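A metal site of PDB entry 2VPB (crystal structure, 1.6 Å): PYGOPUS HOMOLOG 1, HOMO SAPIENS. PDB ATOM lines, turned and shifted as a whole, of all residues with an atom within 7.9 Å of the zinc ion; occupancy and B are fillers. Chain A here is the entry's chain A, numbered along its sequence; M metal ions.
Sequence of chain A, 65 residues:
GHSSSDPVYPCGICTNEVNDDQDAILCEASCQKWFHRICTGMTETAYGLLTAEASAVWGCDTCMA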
ATOM      1  N   PRO A  10      23.800 -17.920 -18.907  1.00  0.00           N
ATOM      2  CA  PRO A  10      24.873 -17.968 -19.899  1.00  0.00           C
ATOM      3  C   PRO A  10      25.967 -18.958 -19.518  1.00  0.00           C
ATOM      4  O   PRO A  10      26.397 -18.994 -18.356  1.00  0.00           O
ATOM      5  CB  PRO A  10      25.427 -16.536 -19.914  1.00  0.00           C
ATOM      6  CG  PRO A  10      25.070 -15.978 -18.564  1.00  0.00           C
ATOM      7  CD  PRO A  10      23.802 -16.656 -18.141  1.00  0.00           C
ATOM      8  N   CYS A  11      26.401 -19.762 -20.475  1.00  0.00           N
ATOM      9  CA  CYS A  11      27.467 -20.748 -20.230  1.00  0.00           C
ATOM     10  C   CYS A  11      28.748 -20.053 -19.802  1.00  0.00           C
ATOM     11  O   CYS A  11      29.184 -19.074 -20.425  1.00  0.00           O
ATOM     12  CB  CYS A  11      27.703 -21.579 -21.493  1.00  0.00           C
ATOM     13  SG  CYS A  11      29.128 -22.721 -21.443  1.00  0.00           S
ATOM     14  N   GLY A  12      29.353 -20.551 -18.725  1.00  0.00           N
ATOM     15  CA  GLY A  12      30.578 -19.952 -18.186  1.00  0.00           C
ATOM     16  C   GLY A  12      31.770 -19.979 -19.128  1.00  0.00           C
ATOM     17  O   GLY A  12      32.770 -19.296 -18.878  1.00  0.00           O
ATOM     18  N   ILE A  13      31.683 -20.777 -20.198  1.00  0.00           N
ATOM     19  CA  ILE A  13      32.747 -20.835 -21.200  1.00  0.00           C
ATOM     20  C   ILE A  13      32.367 -20.087 -22.472  1.00  0.00           C
ATOM     21  O   ILE A  13      33.046 -19.135 -22.862  1.00  0.00           O
ATOM     22  CB  ILE A  13      33.172 -22.299 -21.502  1.00  0.00           C
ATOM     23  CG1 ILE A  13      33.925 -22.891 -20.303  1.00  0.00           C
ATOM     24  CG2 ILE A  13      34.068 -22.363 -22.740  1.00  0.00           C
ATOM     25  CD1 ILE A  13      33.943 -24.409 -20.236  1.00  0.00           C
ATOM     26  N   CYS A  14      31.275 -20.500 -23.117  1.00  0.00           N
ATOM     27  CA  CYS A  14      30.935 -19.958 -24.446  1.00  0.00           C
ATOM     28  C   CYS A  14      30.049 -18.707 -24.432  1.00  0.00           C
ATOM     29  O   CYS A  14      29.875 -18.054 -25.475  1.00  0.00           O
ATOM     30  CB  CYS A  14      30.326 -21.053 -25.328  1.00  0.00           C
ATOM     31  SG  CYS A  14      28.631 -21.446 -24.980  1.00  0.00           S
ATOM     32  N   THR A  15      29.490 -18.388 -23.260  1.00  0.00           N
ATOM     33  CA  THR A  15      28.523 -17.288 -23.056  1.00  0.00           C
ATOM     34  C   THR A  15      27.108 -17.482 -23.642  1.00  0.00           C
ATOM     35  O   THR A  15      26.193 -16.702 -23.357  1.00  0.00           O
ATOM     36  CB  THR A  15      29.085 -15.865 -23.451  1.00  0.00           C
ATOM     37  OG1 THR A  15      29.039 -15.697 -24.876  1.00  0.00           O
ATOM     38  CG2 THR A  15      30.505 -15.651 -22.938  1.00  0.00           C
ATOM     39  N   ASN A  16      26.910 -18.526 -24.453  1.00  0.00           N
ATOM     40  CA  ASN A  16      25.575 -18.815 -24.982  1.00  0.00           C
ATOM     41  C   ASN A  16      24.673 -19.420 -23.924  1.00  0.00           C
ATOM     42  O   ASN A  16      25.149 -20.048 -22.979  1.00  0.00           O
ATOM     43  CB  ASN A  16      25.668 -19.721 -26.216  1.00  0.00           C
ATOM     44  CG  ASN A  16      26.588 -19.161 -27.283  1.00  0.00           C
ATOM     45  OD1 ASN A  16      27.547 -19.816 -27.698  1.00  0.00           O
ATOM     46  ND2 ASN A  16      26.305 -17.940 -27.716  1.00  0.00           N
ATOM     47  N   GLU A  17      23.365 -19.244 -24.080  1.00  0.00           N
ATOM     48  CA  GLU A  17      22.409 -19.745 -23.101  1.00  0.00           C
ATOM     49  C   GLU A  17      22.508 -21.258 -22.936  1.00  0.00           C
ATOM     50  O   GLU A  17      22.647 -21.996 -23.915  1.00  0.00           O
ATOM     51  CB  GLU A  17      20.977 -19.367 -23.494  1.00  0.00           C
ATOM     52  CG  GLU A  17      20.617 -17.924 -23.179  1.00  0.00           C
ATOM     53  CD  GLU A  17      19.207 -17.582 -23.613  1.00  0.00           C
ATOM     54  OE1 GLU A  17      18.316 -18.460 -23.483  1.00  0.00           O
ATOM     55  OE2 GLU A  17      18.993 -16.453 -24.099  1.00  0.00           O
ATOM     56  N   VAL A  18      22.449 -21.703 -21.687  1.00  0.00           N
ATOM     57  CA  VAL A  18      22.365 -23.120 -21.390  1.00  0.00           C
ATOM     58  C   VAL A  18      20.890 -23.513 -21.354  1.00  0.00           C
ATOM     59  O   VAL A  18      20.179 -23.168 -20.407  1.00  0.00           O
ATOM     60  CB  VAL A  18      23.090 -23.460 -20.066  1.00  0.00           C
ATOM     61  CG1 VAL A  18      23.049 -24.946 -19.814  1.00  0.00           C
ATOM     62  CG2 VAL A  18      24.534 -22.983 -20.123  1.00  0.00           C
ATOM     63  N   GLN A  22      19.970 -29.284 -23.661  1.00  0.00           N
ATOM     64  CA  GLN A  22      21.426 -29.483 -23.690  1.00  0.00           C
ATOM     65  C   GLN A  22      21.870 -30.065 -22.354  1.00  0.00           C
ATOM     66  O   GLN A  22      21.250 -29.781 -21.316  1.00  0.00           O
ATOM     67  CB  GLN A  22      22.148 -28.148 -23.959  1.00  0.00           C
ATOM     68  CG  GLN A  22      21.775 -27.502 -25.298  1.00  0.00           C
ATOM     69  CD  GLN A  22      22.251 -26.071 -25.428  1.00  0.00           C
ATOM     70  OE1 GLN A  22      22.037 -25.230 -24.538  1.00  0.00           O
ATOM     71  NE2 GLN A  22      22.896 -25.764 -26.556  1.00  0.00           N
ATOM     72  N   ASP A  23      22.918 -30.884 -22.384  1.00  0.00           N
ATOM     73  CA  ASP A  23      23.514 -31.378 -21.156  1.00  0.00           C
ATOM     74  C   ASP A  23      24.083 -30.158 -20.437  1.00  0.00           C
ATOM     75  O   ASP A  23      24.967 -29.473 -20.966  1.00  0.00           O
ATOM     76  CB  ASP A  23      24.632 -32.390 -21.439  1.00  0.00           C
ATOM     77  CG  ASP A  23      24.120 -33.703 -22.015  1.00  0.00           C
ATOM     78  OD1 ASP A  23      22.904 -34.006 -21.882  1.00  0.00           O
ATOM     79  OD2 ASP A  23      24.948 -34.443 -22.588  1.00  0.00           O
ATOM     80  N   TRP A  34      26.451 -22.106 -14.657  1.00  0.00           N
ATOM     81  CA  TRP A  34      26.090 -23.236 -15.499  1.00  0.00           C
ATOM     82  C   TRP A  34      26.969 -23.231 -16.735  1.00  0.00           C
ATOM     83  O   TRP A  34      27.419 -22.185 -17.206  1.00  0.00           O
ATOM     84  CB  TRP A  34      24.612 -23.156 -15.913  1.00  0.00           C
ATOM     85  CG  TRP A  34      23.668 -23.493 -14.783  1.00  0.00           C
ATOM     86  CD1 TRP A  34      23.071 -22.604 -13.935  1.00  0.00           C
ATOM     87  CD2 TRP A  34      23.215 -24.794 -14.406  1.00  0.00           C
ATOM     88  NE1 TRP A  34      22.269 -23.281 -13.047  1.00  0.00           N
ATOM     89  CE2 TRP A  34      22.341 -24.620 -13.312  1.00  0.00           C
ATOM     90  CE3 TRP A  34      23.468 -26.083 -14.875  1.00  0.00           C
ATOM     91  CZ2 TRP A  34      21.717 -25.704 -12.687  1.00  0.00           C
ATOM     92  CZ3 TRP A  34      22.850 -27.160 -14.253  1.00  0.00           C
ATOM     93  CH2 TRP A  34      21.991 -26.957 -13.162  1.00  0.00           C
ATOM     94  N   PHE A  35      27.219 -24.431 -17.255  1.00  0.00           N
ATOM     95  CA  PHE A  35      28.020 -24.623 -18.462  1.00  0.00           C
ATOM     96  C   PHE A  35      27.338 -25.686 -19.313  1.00  0.00           C
ATOM     97  O   PHE A  35      26.621 -26.535 -18.790  1.00  0.00           O
ATOM     98  CB  PHE A  35      29.430 -25.139 -18.120  1.00  0.00           C
ATOM     99  CG  PHE A  35      30.241 -24.256 -17.195  1.00  0.00           C
ATOM    100  CD1 PHE A  35      31.358 -23.590 -17.677  1.00  0.00           C
ATOM    101  CD2 PHE A  35      29.911 -24.144 -15.825  1.00  0.00           C
ATOM    102  CE1 PHE A  35      32.143 -22.791 -16.838  1.00  0.00           C
ATOM    103  CE2 PHE A  35      30.686 -23.347 -14.976  1.00  0.00           C
ATOM    104  CZ  PHE A  35      31.795 -22.668 -15.474  1.00  0.00           C
ATOM    105  N   HIS A  36      27.538 -25.624 -20.620  1.00  0.00           N
ATOM    106  CA  HIS A  36      27.232 -26.775 -21.470  1.00  0.00           C
ATOM    107  C   HIS A  36      28.264 -27.859 -21.201  1.00  0.00           C
ATOM    108  O   HIS A  36      29.469 -27.574 -21.178  1.00  0.00           O
ATOM    109  CB  HIS A  36      27.356 -26.398 -22.941  1.00  0.00           C
ATOM    110  CG  HIS A  36      26.449 -25.291 -23.365  1.00  0.00           C
ATOM    111  ND1 HIS A  36      26.910 -24.037 -23.710  1.00  0.00           N
ATOM    112  CD2 HIS A  36      25.105 -25.259 -23.545  1.00  0.00           C
ATOM    113  CE1 HIS A  36      25.889 -23.281 -24.059  1.00  0.00           C
ATOM    114  NE2 HIS A  36      24.787 -23.991 -23.966  1.00  0.00           N
ATOM    115  N   ARG A  37      27.793 -29.095 -21.052  1.00  0.00           N
ATOM    116  CA  ARG A  37      28.727 -30.214 -20.922  1.00  0.00           C
ATOM    117  C   ARG A  37      29.800 -30.168 -22.012  1.00  0.00           C
ATOM    118  O   ARG A  37      30.984 -30.299 -21.733  1.00  0.00           O
ATOM    119  CB  ARG A  37      28.024 -31.567 -21.004  1.00  0.00           C
ATOM    120  CG  ARG A  37      29.017 -32.710 -20.980  1.00  0.00           C
ATOM    121  CD  ARG A  37      28.388 -34.015 -21.411  1.00  0.00           C
ATOM    122  NE  ARG A  37      27.837 -33.952 -22.768  1.00  0.00           N
ATOM    123  CZ  ARG A  37      28.552 -33.983 -23.890  1.00  0.00           C
ATOM    124  NH1 ARG A  37      29.881 -34.072 -23.871  1.00  0.00           N
ATOM    125  NH2 ARG A  37      27.925 -33.953 -25.057  1.00  0.00           N
ATOM    126  N   ILE A  38      29.378 -29.974 -23.266  1.00  0.00           N
ATOM    127  CA  ILE A  38      30.351 -30.038 -24.358  1.00  0.00           C
ATOM    128  C   ILE A  38      31.474 -29.002 -24.222  1.00  0.00           C
ATOM    129  O   ILE A  38      32.635 -29.291 -24.541  1.00  0.00           O
ATOM    130  CB  ILE A  38      29.709 -30.039 -25.782  1.00  0.00           C
ATOM    131  CG1 ILE A  38      29.162 -28.683 -26.179  1.00  0.00           C
ATOM    132  CG2 ILE A  38      28.623 -31.066 -25.891  1.00  0.00           C
ATOM    133  CD1 ILE A  38      29.138 -28.507 -27.701  1.00  0.00           C
ATOM    134  N   CYS A  39      31.150 -27.812 -23.705  1.00  0.00           N
ATOM    135  CA  CYS A  39      32.147 -26.761 -23.551  1.00  0.00           C
ATOM    136  C   CYS A  39      33.221 -27.122 -22.534  1.00  0.00           C
ATOM    137  O   CYS A  39      34.363 -26.686 -22.653  1.00  0.00           O
ATOM    138  CB  CYS A  39      31.481 -25.437 -23.173  1.00  0.00           C
ATOM    139  SG  CYS A  39      30.419 -24.838 -24.497  1.00  0.00           S
ATOM    140  N   THR A  40      32.823 -27.881 -21.518  1.00  0.00           N
ATOM    141  CA  THR A  40      33.744 -28.262 -20.454  1.00  0.00           C
ATOM    142  C   THR A  40      34.771 -29.302 -20.880  1.00  0.00           C
ATOM    143  O   THR A  40      35.817 -29.413 -20.246  1.00  0.00           O
ATOM    144  CB  THR A  40      32.997 -28.820 -19.219  1.00  0.00           C
ATOM    145  OG1 THR A  40      32.471 -30.115 -19.528  1.00  0.00           O
ATOM    146  CG2 THR A  40      31.864 -27.888 -18.771  1.00  0.00           C
HETATM  147 ZN    ZN M   1      28.878 -23.328 -23.632  1.00  0.00          ZN
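The side-chain sulfur (SG) of Cys 11 lies close to the backbone NH (N) of Ile 13 (3.4 Å).
The backbone NH of Cys 11 sits at hydrogen-bond distance from the backbone carbonyl oxygen of Asn 16 (2.8 Å).
OD1 of Asn 16 lies close to SG of Cys 14 (3.3 Å).
The backbone carbonyl oxygen of Glu 17 sits at hydrogen-bond distance from a ring nitrogen (NE2) of His 36 (2.9 Å).
NE2 of His 36 lies within hydrogen-bond range of OE1 of Gln 22, 3.1 Å away.
Within 4 Å of the zinc ion: Cys 11, Cys 14, His 36 and Cys 39.
The zinc ion is bound by a ring nitrogen (ND1) of His 36 (2.1 Å), the side-chain sulfur (SG) of Cys 11 (2.3 Å), the side-chain sulfur (SG) of Cys 39 (2.3 Å) and the side-chain sulfur (SG) of Cys 14 (2.3 Å).
The zinc ion has four donor atoms within binding distance.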
